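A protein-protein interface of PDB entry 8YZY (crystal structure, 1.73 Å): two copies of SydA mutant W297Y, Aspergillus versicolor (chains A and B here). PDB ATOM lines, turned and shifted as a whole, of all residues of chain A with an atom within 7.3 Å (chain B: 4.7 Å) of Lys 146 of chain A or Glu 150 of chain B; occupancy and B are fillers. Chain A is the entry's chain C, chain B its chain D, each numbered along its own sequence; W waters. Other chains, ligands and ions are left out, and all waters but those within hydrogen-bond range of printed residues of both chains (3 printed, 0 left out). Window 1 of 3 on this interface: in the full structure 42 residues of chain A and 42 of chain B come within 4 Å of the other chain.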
ATOM      1  N   LEU A 129      35.143  -7.240 -23.453  1.00  0.00           N
ATOM      2  CA  LEU A 129      33.891  -7.914 -23.108  1.00  0.00           C
ATOM      3  C   LEU A 129      33.158  -7.175 -21.993  1.00  0.00           C
ATOM      4  O   LEU A 129      31.921  -7.100 -21.995  1.00  0.00           O
ATOM      5  CB  LEU A 129      34.168  -9.352 -22.692  1.00  0.00           C
ATOM      6  CG  LEU A 129      34.743 -10.216 -23.832  1.00  0.00           C
ATOM      7  CD1 LEU A 129      34.877 -11.643 -23.356  1.00  0.00           C
ATOM      8  CD2 LEU A 129      33.860 -10.156 -25.085  1.00  0.00           C
ATOM      9  N   TYR A 139      20.972  -8.131 -24.587  1.00  0.00           N
ATOM     10  CA  TYR A 139      21.054  -9.411 -25.300  1.00  0.00           C
ATOM     11  C   TYR A 139      22.285  -9.456 -26.197  1.00  0.00           C
ATOM     12  O   TYR A 139      23.045 -10.431 -26.176  1.00  0.00           O
ATOM     13  CB  TYR A 139      19.766  -9.648 -26.103  1.00  0.00           C
ATOM     14  CG  TYR A 139      19.630 -11.023 -26.764  1.00  0.00           C
ATOM     15  CD1 TYR A 139      20.170 -11.276 -28.015  1.00  0.00           C
ATOM     16  CD2 TYR A 139      18.922 -12.046 -26.139  1.00  0.00           C
ATOM     17  CE1 TYR A 139      20.039 -12.545 -28.625  1.00  0.00           C
ATOM     18  CE2 TYR A 139      18.789 -13.309 -26.738  1.00  0.00           C
ATOM     19  CZ  TYR A 139      19.357 -13.543 -27.973  1.00  0.00           C
ATOM     20  OH  TYR A 139      19.225 -14.779 -28.559  1.00  0.00           O
ATOM     21  N   GLY A 140      22.522  -8.391 -26.976  1.00  0.00           N
ATOM     22  CA  GLY A 140      23.703  -8.369 -27.834  1.00  0.00           C
ATOM     23  C   GLY A 140      25.007  -8.461 -27.050  1.00  0.00           C
ATOM     24  O   GLY A 140      25.924  -9.168 -27.453  1.00  0.00           O
ATOM     25  N   SER A 141      25.108  -7.745 -25.916  1.00  0.00           N
ATOM     26  CA  SER A 141      26.332  -7.814 -25.103  1.00  0.00           C
ATOM     27  C   SER A 141      26.570  -9.218 -24.576  1.00  0.00           C
ATOM     28  O   SER A 141      27.703  -9.730 -24.635  1.00  0.00           O
ATOM     29  CB  SER A 141      26.288  -6.848 -23.909  1.00  0.00           C
ATOM     30  OG  SER A 141      25.966  -5.540 -24.307  1.00  0.00           O
ATOM     31  N   SER A 142      25.523  -9.844 -24.018  1.00  0.00           N
ATOM     32  CA  SER A 142      25.666 -11.235 -23.594  1.00  0.00           C
ATOM     33  C   SER A 142      26.121 -12.133 -24.739  1.00  0.00           C
ATOM     34  O   SER A 142      26.886 -13.079 -24.522  1.00  0.00           O
ATOM     35  CB  SER A 142      24.351 -11.782 -23.035  1.00  0.00           C
ATOM     36  OG  SER A 142      23.966 -11.077 -21.866  1.00  0.00           O
ATOM     37  N   MET A 143      25.603 -11.902 -25.952  1.00  0.00           N
ATOM     38  CA  MET A 143      25.911 -12.814 -27.051  1.00  0.00           C
ATOM     39  C   MET A 143      27.364 -12.600 -27.497  1.00  0.00           C
ATOM     40  O   MET A 143      28.055 -13.552 -27.865  1.00  0.00           O
ATOM     41  CB  MET A 143      24.952 -12.557 -28.219  1.00  0.00           C
ATOM     42  CG  MET A 143      23.557 -13.157 -28.006  1.00  0.00           C
ATOM     43  SD  MET A 143      23.468 -14.822 -27.277  1.00  0.00           S
ATOM     44  CE  MET A 143      22.792 -14.402 -25.664  1.00  0.00           C
ATOM     45  N   VAL A 144      27.856 -11.360 -27.458  1.00  0.00           N
ATOM     46  CA  VAL A 144      29.273 -11.141 -27.772  1.00  0.00           C
ATOM     47  C   VAL A 144      30.157 -11.834 -26.734  1.00  0.00           C
ATOM     48  O   VAL A 144      31.163 -12.469 -27.077  1.00  0.00           O
ATOM     49  CB  VAL A 144      29.604  -9.634 -27.872  1.00  0.00           C
ATOM     50  CG1 VAL A 144      31.127  -9.409 -28.007  1.00  0.00           C
ATOM     51  CG2 VAL A 144      28.904  -9.043 -29.069  1.00  0.00           C
ATOM     52  N   ILE A 145      29.796 -11.729 -25.447  1.00  0.00           N
ATOM     53  CA  ILE A 145      30.569 -12.426 -24.416  1.00  0.00           C
ATOM     54  C   ILE A 145      30.570 -13.923 -24.671  1.00  0.00           C
ATOM     55  O   ILE A 145      31.620 -14.590 -24.651  1.00  0.00           O
ATOM     56  CB  ILE A 145      30.012 -12.115 -23.015  1.00  0.00           C
ATOM     57  CG1 ILE A 145      30.214 -10.630 -22.712  1.00  0.00           C
ATOM     58  CG2 ILE A 145      30.740 -12.957 -21.942  1.00  0.00           C
ATOM     59  CD1 ILE A 145      29.475 -10.146 -21.434  1.00  0.00           C
ATOM     60  N   LYS A 146      29.386 -14.493 -24.866  1.00  0.00           N
ATOM     61  CA  LYS A 146      29.359 -15.937 -24.930  1.00  0.00           C
ATOM     62  C   LYS A 146      30.036 -16.422 -26.212  1.00  0.00           C
ATOM     63  O   LYS A 146      30.695 -17.473 -26.207  1.00  0.00           O
ATOM     64  CB  LYS A 146      27.905 -16.438 -24.772  1.00  0.00           C
ATOM     65  CG  LYS A 146      27.017 -16.390 -26.057  1.00  0.00           C
ATOM     66  CD  LYS A 146      27.173 -17.599 -26.975  1.00  0.00           C
ATOM     67  CE  LYS A 146      26.435 -17.394 -28.300  1.00  0.00           C
ATOM     68  NZ  LYS A 146      26.432 -18.622 -29.184  1.00  0.00           N
ATOM     69  N   THR A 147      29.952 -15.628 -27.296  1.00  0.00           N
ATOM     70  CA  THR A 147      30.576 -15.989 -28.566  1.00  0.00           C
ATOM     71  C   THR A 147      32.090 -15.926 -28.454  1.00  0.00           C
ATOM     72  O   THR A 147      32.802 -16.753 -29.033  1.00  0.00           O
ATOM     73  CB  THR A 147      30.085 -15.032 -29.662  1.00  0.00           C
ATOM     74  OG1 THR A 147      28.671 -15.195 -29.807  1.00  0.00           O
ATOM     75  CG2 THR A 147      30.785 -15.294 -31.036  1.00  0.00           C
ATOM     76  N   THR A 148      32.590 -14.943 -27.717  1.00  0.00           N
ATOM     77  CA  THR A 148      34.034 -14.883 -27.481  1.00  0.00           C
ATOM     78  C   THR A 148      34.524 -16.080 -26.661  1.00  0.00           C
ATOM     79  O   THR A 148      35.604 -16.627 -26.940  1.00  0.00           O
ATOM     80  CB  THR A 148      34.375 -13.551 -26.820  1.00  0.00           C
ATOM     81  OG1 THR A 148      33.885 -12.499 -27.659  1.00  0.00           O
ATOM     82  CG2 THR A 148      35.884 -13.411 -26.647  1.00  0.00           C
ATOM     83  N   LEU A 149      33.760 -16.521 -25.652  1.00  0.00           N
ATOM     84  CA  LEU A 149      34.194 -17.734 -24.942  1.00  0.00           C
ATOM     85  C   LEU A 149      34.267 -18.927 -25.887  1.00  0.00           C
ATOM     86  O   LEU A 149      35.226 -19.726 -25.840  1.00  0.00           O
ATOM     87  CB  LEU A 149      33.265 -18.066 -23.792  1.00  0.00           C
ATOM     88  CG  LEU A 149      33.047 -16.939 -22.796  1.00  0.00           C
ATOM     89  CD1 LEU A 149      32.138 -17.416 -21.694  1.00  0.00           C
ATOM     90  CD2 LEU A 149      34.391 -16.473 -22.261  1.00  0.00           C
ATOM     91  N   GLU A 150      33.248 -19.070 -26.746  1.00  0.00           N
ATOM     92  CA  GLU A 150      33.273 -20.169 -27.725  1.00  0.00           C
ATOM     93  C   GLU A 150      34.459 -20.042 -28.675  1.00  0.00           C
ATOM     94  O   GLU A 150      35.066 -21.047 -29.039  1.00  0.00           O
ATOM     95  CB  GLU A 150      31.996 -20.210 -28.553  1.00  0.00           C
ATOM     96  CG  GLU A 150      30.723 -20.443 -27.746  1.00  0.00           C
ATOM     97  CD  GLU A 150      29.501 -20.516 -28.647  1.00  0.00           C
ATOM     98  OE1 GLU A 150      29.093 -19.429 -29.176  1.00  0.00           O
ATOM     99  OE2 GLU A 150      28.876 -21.605 -28.717  1.00  0.00           O
ATOM    100  N   PHE A 151      34.745 -18.836 -29.149  1.00  0.00           N
ATOM    101  CA  PHE A 151      35.839 -18.638 -30.110  1.00  0.00           C
ATOM    102  C   PHE A 151      37.189 -18.998 -29.498  1.00  0.00           C
ATOM    103  O   PHE A 151      38.042 -19.621 -30.151  1.00  0.00           O
ATOM    104  CB  PHE A 151      35.883 -17.172 -30.581  1.00  0.00           C
ATOM    105  CG  PHE A 151      37.096 -16.862 -31.429  1.00  0.00           C
ATOM    106  CD1 PHE A 151      37.131 -17.250 -32.766  1.00  0.00           C
ATOM    107  CD2 PHE A 151      38.200 -16.235 -30.885  1.00  0.00           C
ATOM    108  CE1 PHE A 151      38.261 -16.987 -33.555  1.00  0.00           C
ATOM    109  CE2 PHE A 151      39.316 -15.994 -31.655  1.00  0.00           C
ATOM    110  CZ  PHE A 151      39.360 -16.365 -32.966  1.00  0.00           C
ATOM    111  N   VAL A 152      37.428 -18.578 -28.252  1.00  0.00           N
ATOM    112  CA  VAL A 152      38.722 -18.886 -27.636  1.00  0.00           C
ATOM    113  C   VAL A 152      38.881 -20.401 -27.503  1.00  0.00           C
ATOM    114  O   VAL A 152      39.915 -20.978 -27.883  1.00  0.00           O
ATOM    115  CB  VAL A 152      38.855 -18.172 -26.282  1.00  0.00           C
ATOM    116  CG1 VAL A 152      39.999 -18.763 -25.475  1.00  0.00           C
ATOM    117  CG2 VAL A 152      39.016 -16.651 -26.474  1.00  0.00           C
ATOM    118  N   VAL A 178      30.352 -23.167 -35.910  1.00  0.00           N
ATOM    119  CA  VAL A 178      29.724 -22.223 -34.985  1.00  0.00           C
ATOM    120  C   VAL A 178      30.739 -21.774 -33.943  1.00  0.00           C
ATOM    121  O   VAL A 178      30.878 -20.573 -33.665  1.00  0.00           O
ATOM    122  CB  VAL A 178      28.480 -22.839 -34.326  1.00  0.00           C
ATOM    123  CG1 VAL A 178      28.033 -21.971 -33.105  1.00  0.00           C
ATOM    124  CG2 VAL A 178      27.343 -22.979 -35.334  1.00  0.00           C
ATOM    125  N   LYS A 179      31.489 -22.726 -33.372  1.00  0.00           N
ATOM    126  CA  LYS A 179      32.434 -22.340 -32.314  1.00  0.00           C
ATOM    127  C   LYS A 179      33.545 -21.418 -32.814  1.00  0.00           C
ATOM    128  O   LYS A 179      33.952 -20.504 -32.093  1.00  0.00           O
ATOM    129  CB  LYS A 179      33.048 -23.568 -31.621  1.00  0.00           C
ATOM    130  CG  LYS A 179      32.034 -24.536 -31.009  1.00  0.00           C
ATOM    131  CD  LYS A 179      31.214 -23.904 -29.909  1.00  0.00           C
ATOM    132  CE  LYS A 179      30.415 -24.987 -29.215  1.00  0.00           C
ATOM    133  NZ  LYS A 179      29.135 -24.490 -28.707  1.00  0.00           N
ATOM    134  N   PHE A 182      32.860 -16.982 -34.912  1.00  0.00           N
ATOM    135  CA  PHE A 182      32.659 -15.676 -34.270  1.00  0.00           C
ATOM    136  C   PHE A 182      31.474 -14.904 -34.867  1.00  0.00           C
ATOM    137  O   PHE A 182      31.421 -13.667 -34.759  1.00  0.00           O
ATOM    138  CB  PHE A 182      33.961 -14.838 -34.386  1.00  0.00           C
ATOM    139  CG  PHE A 182      34.169 -13.814 -33.268  1.00  0.00           C
ATOM    140  CD1 PHE A 182      34.140 -14.203 -31.941  1.00  0.00           C
ATOM    141  CD2 PHE A 182      34.449 -12.492 -33.573  1.00  0.00           C
ATOM    142  CE1 PHE A 182      34.322 -13.284 -30.926  1.00  0.00           C
ATOM    143  CE2 PHE A 182      34.647 -11.562 -32.558  1.00  0.00           C
ATOM    144  CZ  PHE A 182      34.568 -11.959 -31.236  1.00  0.00           C
ATOM    145  N   GLU A 184      28.169 -14.426 -34.307  1.00  0.00           N
ATOM    146  CA  GLU A 184      27.149 -13.655 -33.587  1.00  0.00           C
ATOM    147  C   GLU A 184      27.653 -12.282 -33.224  1.00  0.00           C
ATOM    148  O   GLU A 184      26.866 -11.332 -33.168  1.00  0.00           O
ATOM    149  CB  GLU A 184      26.664 -14.384 -32.331  1.00  0.00           C
ATOM    150  CG  GLU A 184      25.513 -15.287 -32.657  1.00  0.00           C
ATOM    151  CD  GLU A 184      25.251 -16.315 -31.564  1.00  0.00           C
ATOM    152  OE1 GLU A 184      25.914 -17.389 -31.592  1.00  0.00           O
ATOM    153  OE2 GLU A 184      24.408 -16.016 -30.680  1.00  0.00           O
ATOM    154  N   THR A 185      28.973 -12.140 -33.035  1.00  0.00           N
ATOM    155  CA  THR A 185      29.525 -10.836 -32.673  1.00  0.00           C
ATOM    156  C   THR A 185      29.289  -9.814 -33.777  1.00  0.00           C
ATOM    157  O   THR A 185      28.919  -8.665 -33.510  1.00  0.00           O
ATOM    158  CB  THR A 185      31.009 -10.995 -32.370  1.00  0.00           C
ATOM    159  OG1 THR A 185      31.133 -11.795 -31.178  1.00  0.00           O
ATOM    160  CG2 THR A 185      31.692  -9.621 -32.155  1.00  0.00           C
ATOM    161  N   LYS B 146      28.980 -20.311 -21.204  1.00  0.00           N
ATOM    162  CA  LYS B 146      28.362 -19.629 -22.333  1.00  0.00           C
ATOM    163  C   LYS B 146      26.895 -20.056 -22.484  1.00  0.00           C
ATOM    164  O   LYS B 146      26.047 -19.225 -22.841  1.00  0.00           O
ATOM    165  CB  LYS B 146      29.202 -19.857 -23.598  1.00  0.00           C
ATOM    166  CG  LYS B 146      28.994 -21.221 -24.265  1.00  0.00           C
ATOM    167  CD  LYS B 146      27.847 -21.225 -25.277  1.00  0.00           C
ATOM    168  CE  LYS B 146      27.466 -22.656 -25.716  1.00  0.00           C
ATOM    169  NZ  LYS B 146      26.419 -22.665 -26.815  1.00  0.00           N
ATOM    170  N   THR B 147      26.574 -21.326 -22.159  1.00  0.00           N
ATOM    171  CA  THR B 147      25.190 -21.808 -22.187  1.00  0.00           C
ATOM    172  C   THR B 147      24.339 -21.106 -21.142  1.00  0.00           C
ATOM    173  O   THR B 147      23.155 -20.807 -21.377  1.00  0.00           O
ATOM    174  CB  THR B 147      25.173 -23.320 -21.941  1.00  0.00           C
ATOM    175  OG1 THR B 147      25.934 -23.961 -22.973  1.00  0.00           O
ATOM    176  CG2 THR B 147      23.717 -23.866 -21.957  1.00  0.00           C
ATOM    177  N   THR B 148      24.915 -20.838 -19.968  1.00  0.00           N
ATOM    178  CA  THR B 148      24.132 -20.136 -18.941  1.00  0.00           C
ATOM    179  C   THR B 148      23.842 -18.701 -19.370  1.00  0.00           C
ATOM    180  O   THR B 148      22.754 -18.171 -19.102  1.00  0.00           O
ATOM    181  CB  THR B 148      24.886 -20.174 -17.608  1.00  0.00           C
ATOM    182  OG1 THR B 148      25.062 -21.546 -17.227  1.00  0.00           O
ATOM    183  CG2 THR B 148      24.112 -19.433 -16.476  1.00  0.00           C
ATOM    184  N   LEU B 149      24.824 -18.047 -20.003  1.00  0.00           N
ATOM    185  CA  LEU B 149      24.574 -16.697 -20.514  1.00  0.00           C
ATOM    186  C   LEU B 149      23.448 -16.700 -21.546  1.00  0.00           C
ATOM    187  O   LEU B 149      22.554 -15.824 -21.528  1.00  0.00           O
ATOM    188  CB  LEU B 149      25.849 -16.115 -21.132  1.00  0.00           C
ATOM    189  CG  LEU B 149      27.051 -16.012 -20.199  1.00  0.00           C
ATOM    190  CD1 LEU B 149      28.174 -15.216 -20.889  1.00  0.00           C
ATOM    191  CD2 LEU B 149      26.635 -15.350 -18.866  1.00  0.00           C
ATOM    192  N   GLU B 150      23.480 -17.683 -22.457  1.00  0.00           N
ATOM    193  CA  GLU B 150      22.408 -17.806 -23.447  1.00  0.00           C
ATOM    194  C   GLU B 150      21.062 -18.027 -22.775  1.00  0.00           C
ATOM    195  O   GLU B 150      20.065 -17.438 -23.181  1.00  0.00           O
ATOM    196  CB  GLU B 150      22.686 -18.965 -24.394  1.00  0.00           C
ATOM    197  CG  GLU B 150      23.878 -18.680 -25.348  1.00  0.00           C
ATOM    198  CD  GLU B 150      24.124 -19.880 -26.267  1.00  0.00           C
ATOM    199  OE1 GLU B 150      24.179 -21.034 -25.739  1.00  0.00           O
ATOM    200  OE2 GLU B 150      24.269 -19.680 -27.492  1.00  0.00           O
ATOM    201  N   PHE B 151      21.016 -18.891 -21.769  1.00  0.00           N
ATOM    202  CA  PHE B 151      19.751 -19.190 -21.098  1.00  0.00           C
ATOM    203  C   PHE B 151      19.179 -17.967 -20.394  1.00  0.00           C
ATOM    204  O   PHE B 151      17.975 -17.697 -20.483  1.00  0.00           O
ATOM    205  CB  PHE B 151      19.942 -20.317 -20.092  1.00  0.00           C
ATOM    206  CG  PHE B 151      18.695 -20.629 -19.309  1.00  0.00           C
ATOM    207  CD1 PHE B 151      17.780 -21.542 -19.816  1.00  0.00           C
ATOM    208  CD2 PHE B 151      18.445 -20.054 -18.072  1.00  0.00           C
ATOM    209  CE1 PHE B 151      16.610 -21.843 -19.117  1.00  0.00           C
ATOM    210  CE2 PHE B 151      17.270 -20.340 -17.374  1.00  0.00           C
ATOM    211  CZ  PHE B 151      16.364 -21.245 -17.885  1.00  0.00           C
ATOM    212  N   VAL B 152      20.010 -17.238 -19.633  1.00  0.00           N
ATOM    213  CA  VAL B 152      19.517 -16.054 -18.917  1.00  0.00           C
ATOM    214  C   VAL B 152      18.919 -15.045 -19.902  1.00  0.00           C
ATOM    215  O   VAL B 152      17.784 -14.540 -19.730  1.00  0.00           O
ATOM    216  CB  VAL B 152      20.654 -15.430 -18.074  1.00  0.00           C
ATOM    217  CG1 VAL B 152      20.241 -14.084 -17.537  1.00  0.00           C
ATOM    218  CG2 VAL B 152      21.017 -16.349 -16.936  1.00  0.00           C
ATOM    219  N   GLU B 153      19.651 -14.764 -20.984  1.00  0.00           N
ATOM    220  CA  GLU B 153      19.145 -13.735 -21.890  1.00  0.00           C
ATOM    221  C   GLU B 153      18.039 -14.250 -22.810  1.00  0.00           C
ATOM    222  O   GLU B 153      17.102 -13.508 -23.141  1.00  0.00           O
ATOM    223  CB  GLU B 153      20.300 -13.154 -22.696  1.00  0.00           C
ATOM    224  CG  GLU B 153      20.939 -11.998 -21.962  1.00  0.00           C
ATOM    225  CD  GLU B 153      19.954 -10.888 -21.639  1.00  0.00           C
ATOM    226  OE1 GLU B 153      19.170 -10.493 -22.529  1.00  0.00           O
ATOM    227  OE2 GLU B 153      19.966 -10.402 -20.489  1.00  0.00           O
ATOM    228  N   GLY B 154      18.125 -15.502 -23.251  1.00  0.00           N
ATOM    229  CA  GLY B 154      17.083 -16.064 -24.066  1.00  0.00           C
ATOM    230  C   GLY B 154      15.787 -16.198 -23.312  1.00  0.00           C
ATOM    231  O   GLY B 154      14.713 -16.019 -23.888  1.00  0.00           O
ATOM    232  N   THR B 155      15.859 -16.504 -22.017  1.00  0.00           N
ATOM    233  CA  THR B 155      14.652 -16.490 -21.211  1.00  0.00           C
ATOM    234  C   THR B 155      14.044 -15.105 -21.202  1.00  0.00           C
ATOM    235  O   THR B 155      12.827 -14.954 -21.392  1.00  0.00           O
ATOM    236  CB  THR B 155      14.976 -16.968 -19.797  1.00  0.00           C
ATOM    237  OG1 THR B 155      15.349 -18.341 -19.883  1.00  0.00           O
ATOM    238  CG2 THR B 155      13.760 -16.811 -18.875  1.00  0.00           C
ATOM    239  N   LYS B 179      18.799 -21.451 -27.573  1.00  0.00           N
ATOM    240  CA  LYS B 179      19.122 -20.455 -26.539  1.00  0.00           C
ATOM    241  C   LYS B 179      18.454 -20.782 -25.205  1.00  0.00           C
ATOM    242  O   LYS B 179      19.012 -20.483 -24.145  1.00  0.00           O
ATOM    243  CB  LYS B 179      18.727 -19.022 -26.943  1.00  0.00           C
ATOM    244  CG  LYS B 179      19.428 -18.453 -28.170  1.00  0.00           C
ATOM    245  CD  LYS B 179      20.934 -18.433 -27.985  1.00  0.00           C
ATOM    246  CE  LYS B 179      21.549 -17.616 -29.103  1.00  0.00           C
ATOM    247  NZ  LYS B 179      22.916 -18.037 -29.508  1.00  0.00           N
HETATM  248  O   HOH W   1      22.730 -11.012 -18.753  1.00  0.00           O
HETATM  249  O   HOH W   2      23.193 -13.384 -19.804  1.00  0.00           O
HETATM  250  O   HOH W   3      26.604 -21.656 -29.587  1.00  0.00           O
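Hydrophobic or aromatic side chains of chain B that line the printed part of chain A: Leu 149. Of the 20 printed residues of chain A, 8 touch a printed residue of chain B. Printed residues of chain A that touch a printed residue of chain B: Tyr 139, Ser 142, Met 143, Ile 145, Lys 146, Glu 150, Lys 179 and Glu 184. Hydrophobic or aromatic side chains of chain A within 4 Å of the printed part of chain B: Tyr 139, Met 143 and Ile 145. Among the printed residues, 11 pairs touch across the chains. Among the printed residues, Asp or Glu carboxylates within 4 Å of a Lys or Arg side-chain nitrogen of the other chain: Lys 146 of chain A with Glu 150 of chain B (2.9 Å), Glu 150 of chain A with Lys 146 of chain B (3.3 Å) and Glu 184 of chain A with Lys 179 of chain B (2.8 Å).
OE1 of Glu 153 of chain B touches CA of Tyr 139 of chain A (3.5 Å). Tyr 139 of chain A touches Lys 179 of chain B (OH to CG, 3.7 Å). OG of Ser 142 of chain A touches CG of Glu 153 of chain B, 3.2 Å away. Met 143 of chain A touches Lys 179 of chain B (SD to CE, 3.9 Å). CG2 of Ile 145 of chain A touches CD1 of Leu 149 of chain B, at 3.6 Å. O of Lys 146 of chain A touches CB of Lys 146 of chain B, at 3.8 Å. Lys 146 of chain A touches Lys 179 of chain B (NZ to NZ, 3.6 Å). Lys 146 of chain B touches Lys 179 of chain A (NZ to NZ, 3.8 Å).
Of the printed residues of chain B, Ile 145 of chain A touches Leu 149. Of the printed residues of chain A, Lys 179 of chain B touches Tyr 139, Met 143, Lys 146 and Glu 184. Printed residues of chain B within 4 Å of Met 143 of chain A: Lys 179 (3.9 Å). Phe 151 of chain A touches none of the printed residues of chain B. Val 152 of chain B touches none of the printed residues of chain A. The nearest residue of chain B that does not touch Lys 146 of chain A is Leu 149 of chain B (4.1 Å). The nearest printed residue of chain A that does not touch Glu 153 of chain B is Met 143 of chain A (4.1 Å).
O of Met 143 of chain A is in hydrogen-bond range of OG1 of Thr 147 of chain A (2.6 Å). The side-chain carboxylate (OE2) of Glu 150 of chain A lies within salt-bridge range of the side-chain amino group (NZ) of Lys 179 of chain A. O of Lys 179 of chain A sits close to N of Phe 151 of chain A, 3.5 Å away. NZ of Lys 146 of chain B lies within salt-bridge range of OE1 of Glu 150 of chain B, at 3.0 Å. The side-chain carboxylate (OE2) of Glu 150 of chain B lies within salt-bridge range of the side-chain amino group (NZ) of Lys 179 of chain B (2.9 Å). N of Phe 151 of chain B lies close to O of Lys 179 of chain B, 3.5 Å away.
OE2 of Glu 150 of chain B lies within salt-bridge range of NZ of Lys 146 of chain A (2.9 Å). The side-chain carboxylate (OE2) of Glu 150 of chain A lies within salt-bridge range of the side-chain amino group (NZ) of Lys 146 of chain B (3.3 Å). The side-chain amino group (NZ) of Lys 179 of chain B is in salt-bridge range of the side-chain carboxylate (OE2) of Glu 184 of chain A (2.8 Å).
Water W3 lies within hydrogen-bond range of OE2 of Glu 150 of chain A (2.4 Å), NZ of Lys 146 of chain B (3.0 Å) and NZ of Lys 146 of chain A (3.1 Å). Water W2 lies within hydrogen-bond range of the backbone carbonyl oxygen of Leu 149 of chain B and the side-chain hydroxyl of Ser 142 of chain A. Water W1 lies within hydrogen-bond range of OE2 of Glu 153 of chain B and OG of Ser 142 of chain A.
Lys 146 of chain B touches its own counterpart, Lys 146 of chain A. Lys 146 of chain A touches Glu 150 of chain B, and with the chains exchanged Glu 150 of chain A touches Lys 146 of chain B. Lys 146 of chain A touches Lys 179 of chain B, and with the chains exchanged Lys 179 of chain A touches Lys 146 of chain B. Positions printed for both chains: 146, 147, 148, 149, 150, 151, 152 and 179. Of the 11 pairs that touch across the chains among the printed residues, 5 have their exchanged pair printed and touching as well.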
